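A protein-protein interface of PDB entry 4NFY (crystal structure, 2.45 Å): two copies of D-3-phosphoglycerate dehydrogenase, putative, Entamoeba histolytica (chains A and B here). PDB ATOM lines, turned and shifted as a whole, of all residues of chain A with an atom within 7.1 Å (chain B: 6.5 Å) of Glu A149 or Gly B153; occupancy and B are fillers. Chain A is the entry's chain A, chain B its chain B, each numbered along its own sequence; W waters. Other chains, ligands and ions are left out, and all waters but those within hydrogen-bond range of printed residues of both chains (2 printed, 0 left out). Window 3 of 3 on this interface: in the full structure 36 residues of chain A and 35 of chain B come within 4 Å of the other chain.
Among the printed residues, merely in contact across the chains: Asn A104 with Lys B131 (3.3 Å), Arg A146 with Lys B131 (3.5 Å), Glu A149 with Gly B153 (3.9 Å), Ile A150 with Ile B154 (3.4 Å), Gly A153 with Gly B153 (3.8 Å), Ile A154 with Ile B150 (3.4 Å) and Ile A154 with Ile B154 (3.6 Å).
Of the 10 printed residues of chain B, 4 touch a printed residue of chain A.
Hydrophobic or aromatic side chains of chain B within 4 Å of the printed part of chain A: Ile B150 and Ile B154.
Among the printed residues, 8 pairs touch across the chains.
Water W2 lies within hydrogen-bond range of the backbone carbonyl oxygen of Glu A149, the backbone carbonyl oxygen of Gly B153 and the backbone NH of Gly A153.
Water W1 lies within hydrogen-bond range of the guanidinium group of Arg A146, the backbone carbonyl oxygen of Gly B153 and the backbone NH of Gly B155.
The guanidinium group of Arg A146 lies within hydrogen-bond range of the side-chain amide oxygen of Asn A104 (2.7 Å).
NH1 of Arg A146 is in salt-bridge range of OE1 of Glu A149 (2.9 Å).
The guanidinium group (NH2) of Arg A146 is in hydrogen-bond range of the backbone carbonyl oxygen (O) of Ile B154 (3.2 Å).
Of the printed residues of chain B, Asn A104 touches Lys B131 (3.3 Å).
Printed residues of chain B within 4 Å of Arg A146: Lys B131 (3.5 Å) and Ile B154 (3.2 Å).
Of chain B, only Gly B153 (3.9 Å) comes within 4 Å of Glu A149.
Gly B153 touches just these residues of chain A: Glu A149 and Gly A153.
The nearest residue of chain B that does not touch Glu A149 is Ile B154 (5.8 Å).
Glu A149 touches Gly B153, but with the chains exchanged Gly A153 does not touch Glu B149 (4.3 Å).
Ile A150 touches Ile B154, and with the chains exchanged Ile A154 touches Ile B150.
Gly A153 touches its own counterpart, Gly B153.
Ile B154 touches its own counterpart, Ile A154.
Of the 8 pairs that touch across the chains among the printed residues, 4 have their exchanged pair printed and touching as well.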
ATOM      1  N   ARG A 103     -14.549  11.914 -20.802  1.00  0.00           N
ATOM      2  CA  ARG A 103     -15.153  13.093 -20.181  1.00  0.00           C
ATOM      3  C   ARG A 103     -14.168  13.889 -19.327  1.00  0.00           C
ATOM      4  O   ARG A 103     -14.141  15.133 -19.399  1.00  0.00           O
ATOM      5  CB  ARG A 103     -16.387  12.710 -19.354  1.00  0.00           C
ATOM      6  CG  ARG A 103     -16.105  11.990 -18.039  1.00  0.00           C
ATOM      7  CD  ARG A 103     -17.391  11.576 -17.327  1.00  0.00           C
ATOM      8  NE  ARG A 103     -17.979  10.386 -17.937  1.00  0.00           N
ATOM      9  CZ  ARG A 103     -18.842   9.557 -17.344  1.00  0.00           C
ATOM     10  NH1 ARG A 103     -19.251   9.761 -16.090  1.00  0.00           N
ATOM     11  NH2 ARG A 103     -19.307   8.507 -18.015  1.00  0.00           N
ATOM     12  N   ASN A 104     -13.353  13.185 -18.544  1.00  0.00           N
ATOM     13  CA  ASN A 104     -12.411  13.858 -17.671  1.00  0.00           C
ATOM     14  C   ASN A 104     -11.264  14.498 -18.456  1.00  0.00           C
ATOM     15  O   ASN A 104     -10.773  15.566 -18.076  1.00  0.00           O
ATOM     16  CB  ASN A 104     -11.869  12.923 -16.591  1.00  0.00           C
ATOM     17  CG  ASN A 104     -11.059  13.670 -15.560  1.00  0.00           C
ATOM     18  OD1 ASN A 104     -11.585  14.498 -14.835  1.00  0.00           O
ATOM     19  ND2 ASN A 104      -9.763  13.413 -15.521  1.00  0.00           N
ATOM     20  N   ILE A 111     -10.745  23.208 -18.106  1.00  0.00           N
ATOM     21  CA  ILE A 111     -10.314  23.949 -16.917  1.00  0.00           C
ATOM     22  C   ILE A 111      -8.923  24.532 -17.115  1.00  0.00           C
ATOM     23  O   ILE A 111      -8.652  25.672 -16.735  1.00  0.00           O
ATOM     24  CB  ILE A 111     -10.341  23.061 -15.642  1.00  0.00           C
ATOM     25  CG1 ILE A 111     -11.767  22.585 -15.325  1.00  0.00           C
ATOM     26  CG2 ILE A 111      -9.773  23.806 -14.445  1.00  0.00           C
ATOM     27  CD1 ILE A 111     -12.684  23.655 -14.743  1.00  0.00           C
ATOM     28  N   ILE A 137     -22.319  26.853 -17.655  1.00  0.00           N
ATOM     29  CA  ILE A 137     -22.061  25.625 -18.381  1.00  0.00           C
ATOM     30  C   ILE A 137     -23.160  25.373 -19.404  1.00  0.00           C
ATOM     31  O   ILE A 137     -24.323  25.206 -19.034  1.00  0.00           O
ATOM     32  CB  ILE A 137     -22.003  24.411 -17.432  1.00  0.00           C
ATOM     33  CG1 ILE A 137     -21.012  24.657 -16.304  1.00  0.00           C
ATOM     34  CG2 ILE A 137     -21.591  23.148 -18.192  1.00  0.00           C
ATOM     35  CD1 ILE A 137     -20.938  23.519 -15.305  1.00  0.00           C
ATOM     36  N   VAL A 143     -19.411  15.586 -20.276  1.00  0.00           N
ATOM     37  CA  VAL A 143     -18.356  16.591 -20.146  1.00  0.00           C
ATOM     38  C   VAL A 143     -18.815  17.702 -19.206  1.00  0.00           C
ATOM     39  O   VAL A 143     -18.163  18.014 -18.202  1.00  0.00           O
ATOM     40  CB  VAL A 143     -18.008  17.204 -21.531  1.00  0.00           C
ATOM     41  CG1 VAL A 143     -17.063  18.384 -21.391  1.00  0.00           C
ATOM     42  CG2 VAL A 143     -17.412  16.148 -22.454  1.00  0.00           C
ATOM     43  N   GLY A 144     -19.955  18.286 -19.545  1.00  0.00           N
ATOM     44  CA  GLY A 144     -20.548  19.342 -18.746  1.00  0.00           C
ATOM     45  C   GLY A 144     -20.630  18.995 -17.282  1.00  0.00           C
ATOM     46  O   GLY A 144     -20.305  19.818 -16.462  1.00  0.00           O
ATOM     47  N   LYS A 145     -21.069  17.784 -16.946  1.00  0.00           N
ATOM     48  CA  LYS A 145     -21.183  17.384 -15.535  1.00  0.00           C
ATOM     49  C   LYS A 145     -19.831  17.334 -14.827  1.00  0.00           C
ATOM     50  O   LYS A 145     -19.712  17.734 -13.680  1.00  0.00           O
ATOM     51  CB  LYS A 145     -21.849  16.017 -15.397  1.00  0.00           C
ATOM     52  CG  LYS A 145     -23.349  16.017 -15.577  1.00  0.00           C
ATOM     53  CD  LYS A 145     -23.891  14.592 -15.559  1.00  0.00           C
ATOM     54  CE  LYS A 145     -25.390  14.565 -15.839  1.00  0.00           C
ATOM     55  NZ  LYS A 145     -25.813  13.275 -16.453  1.00  0.00           N
ATOM     56  N   ARG A 146     -18.821  16.812 -15.514  1.00  0.00           N
ATOM     57  CA  ARG A 146     -17.489  16.729 -14.947  1.00  0.00           C
ATOM     58  C   ARG A 146     -16.854  18.113 -14.796  1.00  0.00           C
ATOM     59  O   ARG A 146     -16.116  18.354 -13.835  1.00  0.00           O
ATOM     60  CB  ARG A 146     -16.603  15.821 -15.805  1.00  0.00           C
ATOM     61  CG  ARG A 146     -15.187  15.650 -15.287  1.00  0.00           C
ATOM     62  CD  ARG A 146     -15.131  15.005 -13.912  1.00  0.00           C
ATOM     63  NE  ARG A 146     -13.791  15.173 -13.361  1.00  0.00           N
ATOM     64  CZ  ARG A 146     -13.480  15.241 -12.070  1.00  0.00           C
ATOM     65  NH1 ARG A 146     -14.412  15.126 -11.112  1.00  0.00           N
ATOM     66  NH2 ARG A 146     -12.204  15.429 -11.731  1.00  0.00           N
ATOM     67  N   VAL A 147     -17.140  19.016 -15.737  1.00  0.00           N
ATOM     68  CA  VAL A 147     -16.631  20.391 -15.651  1.00  0.00           C
ATOM     69  C   VAL A 147     -17.206  21.092 -14.426  1.00  0.00           C
ATOM     70  O   VAL A 147     -16.486  21.778 -13.694  1.00  0.00           O
ATOM     71  CB  VAL A 147     -16.908  21.189 -16.936  1.00  0.00           C
ATOM     72  CG1 VAL A 147     -16.687  22.681 -16.721  1.00  0.00           C
ATOM     73  CG2 VAL A 147     -16.004  20.675 -18.054  1.00  0.00           C
ATOM     74  N   LYS A 148     -18.496  20.885 -14.200  1.00  0.00           N
ATOM     75  CA  LYS A 148     -19.162  21.341 -12.985  1.00  0.00           C
ATOM     76  C   LYS A 148     -18.437  20.855 -11.728  1.00  0.00           C
ATOM     77  O   LYS A 148     -18.135  21.655 -10.846  1.00  0.00           O
ATOM     78  CB  LYS A 148     -20.614  20.867 -12.985  1.00  0.00           C
ATOM     79  CG  LYS A 148     -21.423  21.291 -11.776  1.00  0.00           C
ATOM     80  CD  LYS A 148     -22.915  21.122 -12.039  1.00  0.00           C
ATOM     81  CE  LYS A 148     -23.679  20.690 -10.791  1.00  0.00           C
ATOM     82  NZ  LYS A 148     -23.405  21.589  -9.644  1.00  0.00           N
ATOM     83  N   GLU A 149     -18.132  19.559 -11.663  1.00  0.00           N
ATOM     84  CA  GLU A 149     -17.435  18.984 -10.496  1.00  0.00           C
ATOM     85  C   GLU A 149     -16.063  19.600 -10.268  1.00  0.00           C
ATOM     86  O   GLU A 149     -15.679  19.858  -9.130  1.00  0.00           O
ATOM     87  CB  GLU A 149     -17.273  17.465 -10.637  1.00  0.00           C
ATOM     88  CG  GLU A 149     -18.569  16.684 -10.549  1.00  0.00           C
ATOM     89  CD  GLU A 149     -18.419  15.210 -10.925  1.00  0.00           C
ATOM     90  OE1 GLU A 149     -17.296  14.735 -11.219  1.00  0.00           O
ATOM     91  OE2 GLU A 149     -19.455  14.515 -10.922  1.00  0.00           O
ATOM     92  N   ILE A 150     -15.320  19.833 -11.347  1.00  0.00           N
ATOM     93  CA  ILE A 150     -13.970  20.375 -11.234  1.00  0.00           C
ATOM     94  C   ILE A 150     -14.053  21.863 -10.908  1.00  0.00           C
ATOM     95  O   ILE A 150     -13.378  22.352  -9.994  1.00  0.00           O
ATOM     96  CB  ILE A 150     -13.138  20.157 -12.521  1.00  0.00           C
ATOM     97  CG1 ILE A 150     -12.984  18.665 -12.840  1.00  0.00           C
ATOM     98  CG2 ILE A 150     -11.756  20.762 -12.345  1.00  0.00           C
ATOM     99  CD1 ILE A 150     -12.295  18.370 -14.163  1.00  0.00           C
ATOM    100  N   ALA A 151     -14.904  22.574 -11.643  1.00  0.00           N
ATOM    101  CA  ALA A 151     -15.111  24.011 -11.433  1.00  0.00           C
ATOM    102  C   ALA A 151     -15.546  24.323 -10.011  1.00  0.00           C
ATOM    103  O   ALA A 151     -15.035  25.237  -9.392  1.00  0.00           O
ATOM    104  CB  ALA A 151     -16.140  24.545 -12.421  1.00  0.00           C
ATOM    105  N   GLU A 152     -16.481  23.556  -9.480  1.00  0.00           N
ATOM    106  CA  GLU A 152     -16.832  23.691  -8.067  1.00  0.00           C
ATOM    107  C   GLU A 152     -15.641  23.411  -7.161  1.00  0.00           C
ATOM    108  O   GLU A 152     -15.416  24.144  -6.198  1.00  0.00           O
ATOM    109  CB  GLU A 152     -18.007  22.787  -7.709  1.00  0.00           C
ATOM    110  CG  GLU A 152     -19.295  23.355  -8.250  1.00  0.00           C
ATOM    111  CD  GLU A 152     -20.504  22.550  -7.877  1.00  0.00           C
ATOM    112  OE1 GLU A 152     -20.443  21.298  -8.004  1.00  0.00           O
ATOM    113  OE2 GLU A 152     -21.520  23.188  -7.484  1.00  0.00           O
ATOM    114  N   GLY A 153     -14.865  22.379  -7.490  1.00  0.00           N
ATOM    115  CA  GLY A 153     -13.708  22.006  -6.691  1.00  0.00           C
ATOM    116  C   GLY A 153     -12.772  23.178  -6.517  1.00  0.00           C
ATOM    117  O   GLY A 153     -12.282  23.461  -5.421  1.00  0.00           O
ATOM    118  N   ILE A 154     -12.544  23.888  -7.609  1.00  0.00           N
ATOM    119  CA  ILE A 154     -11.652  25.021  -7.578  1.00  0.00           C
ATOM    120  C   ILE A 154     -12.375  26.310  -7.179  1.00  0.00           C
ATOM    121  O   ILE A 154     -11.792  27.378  -7.221  1.00  0.00           O
ATOM    122  CB  ILE A 154     -10.891  25.136  -8.906  1.00  0.00           C
ATOM    123  CG1 ILE A 154     -11.733  25.753 -10.014  1.00  0.00           C
ATOM    124  CG2 ILE A 154     -10.456  23.753  -9.357  1.00  0.00           C
ATOM    125  CD1 ILE A 154     -11.014  25.802 -11.343  1.00  0.00           C
ATOM    126  N   GLY A 155     -13.646  26.213  -6.802  1.00  0.00           N
ATOM    127  CA  GLY A 155     -14.339  27.303  -6.124  1.00  0.00           C
ATOM    128  C   GLY A 155     -15.069  28.289  -7.015  1.00  0.00           C
ATOM    129  O   GLY A 155     -15.200  29.448  -6.661  1.00  0.00           O
ATOM    130  N   ILE A 158     -21.799  28.070 -10.064  1.00  0.00           N
ATOM    131  CA  ILE A 158     -22.244  27.386 -11.267  1.00  0.00           C
ATOM    132  C   ILE A 158     -23.675  27.736 -11.662  1.00  0.00           C
ATOM    133  O   ILE A 158     -24.584  27.758 -10.820  1.00  0.00           O
ATOM    134  CB  ILE A 158     -22.186  25.862 -11.076  1.00  0.00           C
ATOM    135  CG1 ILE A 158     -20.781  25.414 -10.659  1.00  0.00           C
ATOM    136  CG2 ILE A 158     -22.617  25.141 -12.345  1.00  0.00           C
ATOM    137  CD1 ILE A 158     -19.697  25.613 -11.704  1.00  0.00           C
ATOM    138  N   LYS B 131      -6.489  13.859 -12.490  1.00  0.00           N
ATOM    139  CA  LYS B 131      -7.424  13.071 -11.709  1.00  0.00           C
ATOM    140  C   LYS B 131      -6.849  11.690 -11.417  1.00  0.00           C
ATOM    141  O   LYS B 131      -6.377  11.013 -12.313  1.00  0.00           O
ATOM    142  CB  LYS B 131      -8.753  12.936 -12.453  1.00  0.00           C
ATOM    143  CG  LYS B 131      -9.791  12.105 -11.711  1.00  0.00           C
ATOM    144  CD  LYS B 131     -11.159  12.182 -12.361  1.00  0.00           C
ATOM    145  CE  LYS B 131     -12.193  11.372 -11.587  1.00  0.00           C
ATOM    146  NZ  LYS B 131     -11.973   9.902 -11.729  1.00  0.00           N
ATOM    147  N   LYS B 148      -3.351  22.190  -2.278  1.00  0.00           N
ATOM    148  CA  LYS B 148      -3.988  20.984  -1.733  1.00  0.00           C
ATOM    149  C   LYS B 148      -5.493  20.997  -1.950  1.00  0.00           C
ATOM    150  O   LYS B 148      -6.059  20.011  -2.420  1.00  0.00           O
ATOM    151  CB  LYS B 148      -3.685  20.852  -0.248  1.00  0.00           C
ATOM    152  CG  LYS B 148      -4.121  19.539   0.369  1.00  0.00           C
ATOM    153  CD  LYS B 148      -3.295  19.249   1.623  1.00  0.00           C
ATOM    154  CE  LYS B 148      -3.720  17.962   2.318  1.00  0.00           C
ATOM    155  NZ  LYS B 148      -5.167  17.983   2.672  1.00  0.00           N
ATOM    156  N   GLU B 149      -6.141  22.119  -1.640  1.00  0.00           N
ATOM    157  CA  GLU B 149      -7.600  22.216  -1.803  1.00  0.00           C
ATOM    158  C   GLU B 149      -8.036  22.088  -3.252  1.00  0.00           C
ATOM    159  O   GLU B 149      -8.987  21.376  -3.558  1.00  0.00           O
ATOM    160  CB  GLU B 149      -8.126  23.528  -1.236  1.00  0.00           C
ATOM    161  CG  GLU B 149      -8.045  23.609   0.275  1.00  0.00           C
ATOM    162  CD  GLU B 149      -8.278  25.010   0.812  1.00  0.00           C
ATOM    163  OE1 GLU B 149      -8.616  25.926   0.036  1.00  0.00           O
ATOM    164  OE2 GLU B 149      -8.123  25.192   2.032  1.00  0.00           O
ATOM    165  N   ILE B 150      -7.334  22.761  -4.152  1.00  0.00           N
ATOM    166  CA  ILE B 150      -7.699  22.714  -5.573  1.00  0.00           C
ATOM    167  C   ILE B 150      -7.434  21.323  -6.151  1.00  0.00           C
ATOM    168  O   ILE B 150      -8.287  20.741  -6.835  1.00  0.00           O
ATOM    169  CB  ILE B 150      -6.947  23.769  -6.418  1.00  0.00           C
ATOM    170  CG1 ILE B 150      -7.200  25.183  -5.886  1.00  0.00           C
ATOM    171  CG2 ILE B 150      -7.420  23.684  -7.858  1.00  0.00           C
ATOM    172  CD1 ILE B 150      -6.504  26.280  -6.669  1.00  0.00           C
ATOM    173  N   ALA B 151      -6.251  20.789  -5.854  1.00  0.00           N
ATOM    174  CA  ALA B 151      -5.863  19.470  -6.331  1.00  0.00           C
ATOM    175  C   ALA B 151      -6.812  18.410  -5.812  1.00  0.00           C
ATOM    176  O   ALA B 151      -7.176  17.512  -6.542  1.00  0.00           O
ATOM    177  CB  ALA B 151      -4.426  19.150  -5.932  1.00  0.00           C
ATOM    178  N   GLU B 152      -7.226  18.502  -4.559  1.00  0.00           N
ATOM    179  CA  GLU B 152      -8.267  17.588  -4.070  1.00  0.00           C
ATOM    180  C   GLU B 152      -9.564  17.757  -4.865  1.00  0.00           C
ATOM    181  O   GLU B 152     -10.144  16.773  -5.310  1.00  0.00           O
ATOM    182  CB  GLU B 152      -8.508  17.764  -2.571  1.00  0.00           C
ATOM    183  CG  GLU B 152      -7.623  16.857  -1.731  1.00  0.00           C
ATOM    184  CD  GLU B 152      -7.468  17.315  -0.298  1.00  0.00           C
ATOM    185  OE1 GLU B 152      -6.798  16.591   0.475  1.00  0.00           O
ATOM    186  OE2 GLU B 152      -7.997  18.397   0.056  1.00  0.00           O
ATOM    187  N   GLY B 153      -9.982  18.999  -5.084  1.00  0.00           N
ATOM    188  CA  GLY B 153     -11.232  19.287  -5.790  1.00  0.00           C
ATOM    189  C   GLY B 153     -11.334  18.647  -7.163  1.00  0.00           C
ATOM    190  O   GLY B 153     -12.425  18.307  -7.631  1.00  0.00           O
ATOM    191  N   ILE B 154     -10.189  18.479  -7.808  1.00  0.00           N
ATOM    192  CA  ILE B 154     -10.136  17.915  -9.141  1.00  0.00           C
ATOM    193  C   ILE B 154      -9.684  16.449  -9.149  1.00  0.00           C
ATOM    194  O   ILE B 154      -9.431  15.890 -10.194  1.00  0.00           O
ATOM    195  CB  ILE B 154      -9.268  18.811 -10.036  1.00  0.00           C
ATOM    196  CG1 ILE B 154      -7.777  18.573  -9.823  1.00  0.00           C
ATOM    197  CG2 ILE B 154      -9.581  20.276  -9.742  1.00  0.00           C
ATOM    198  CD1 ILE B 154      -6.901  19.618 -10.468  1.00  0.00           C
ATOM    199  N   GLY B 155      -9.600  15.825  -7.977  1.00  0.00           N
ATOM    200  CA  GLY B 155      -9.468  14.375  -7.875  1.00  0.00           C
ATOM    201  C   GLY B 155      -8.066  13.810  -7.747  1.00  0.00           C
ATOM    202  O   GLY B 155      -7.849  12.631  -7.984  1.00  0.00           O
ATOM    203  N   MET B 156      -7.105  14.636  -7.373  1.00  0.00           N
ATOM    204  CA  MET B 156      -5.763  14.152  -7.108  1.00  0.00           C
ATOM    205  C   MET B 156      -5.657  13.636  -5.678  1.00  0.00           C
ATOM    206  O   MET B 156      -6.333  14.126  -4.768  1.00  0.00           O
ATOM    207  CB  MET B 156      -4.749  15.269  -7.309  1.00  0.00           C
ATOM    208  CG  MET B 156      -4.801  15.895  -8.685  1.00  0.00           C
ATOM    209  SD  MET B 156      -3.329  16.866  -9.018  1.00  0.00           S
ATOM    210  CE  MET B 156      -2.174  15.565  -9.413  1.00  0.00           C
HETATM  211  O   HOH W   1     -12.858  15.239  -8.697  1.00  0.00           O
HETATM  212  O   HOH W   2     -15.272  19.061  -6.495  1.00  0.00           O
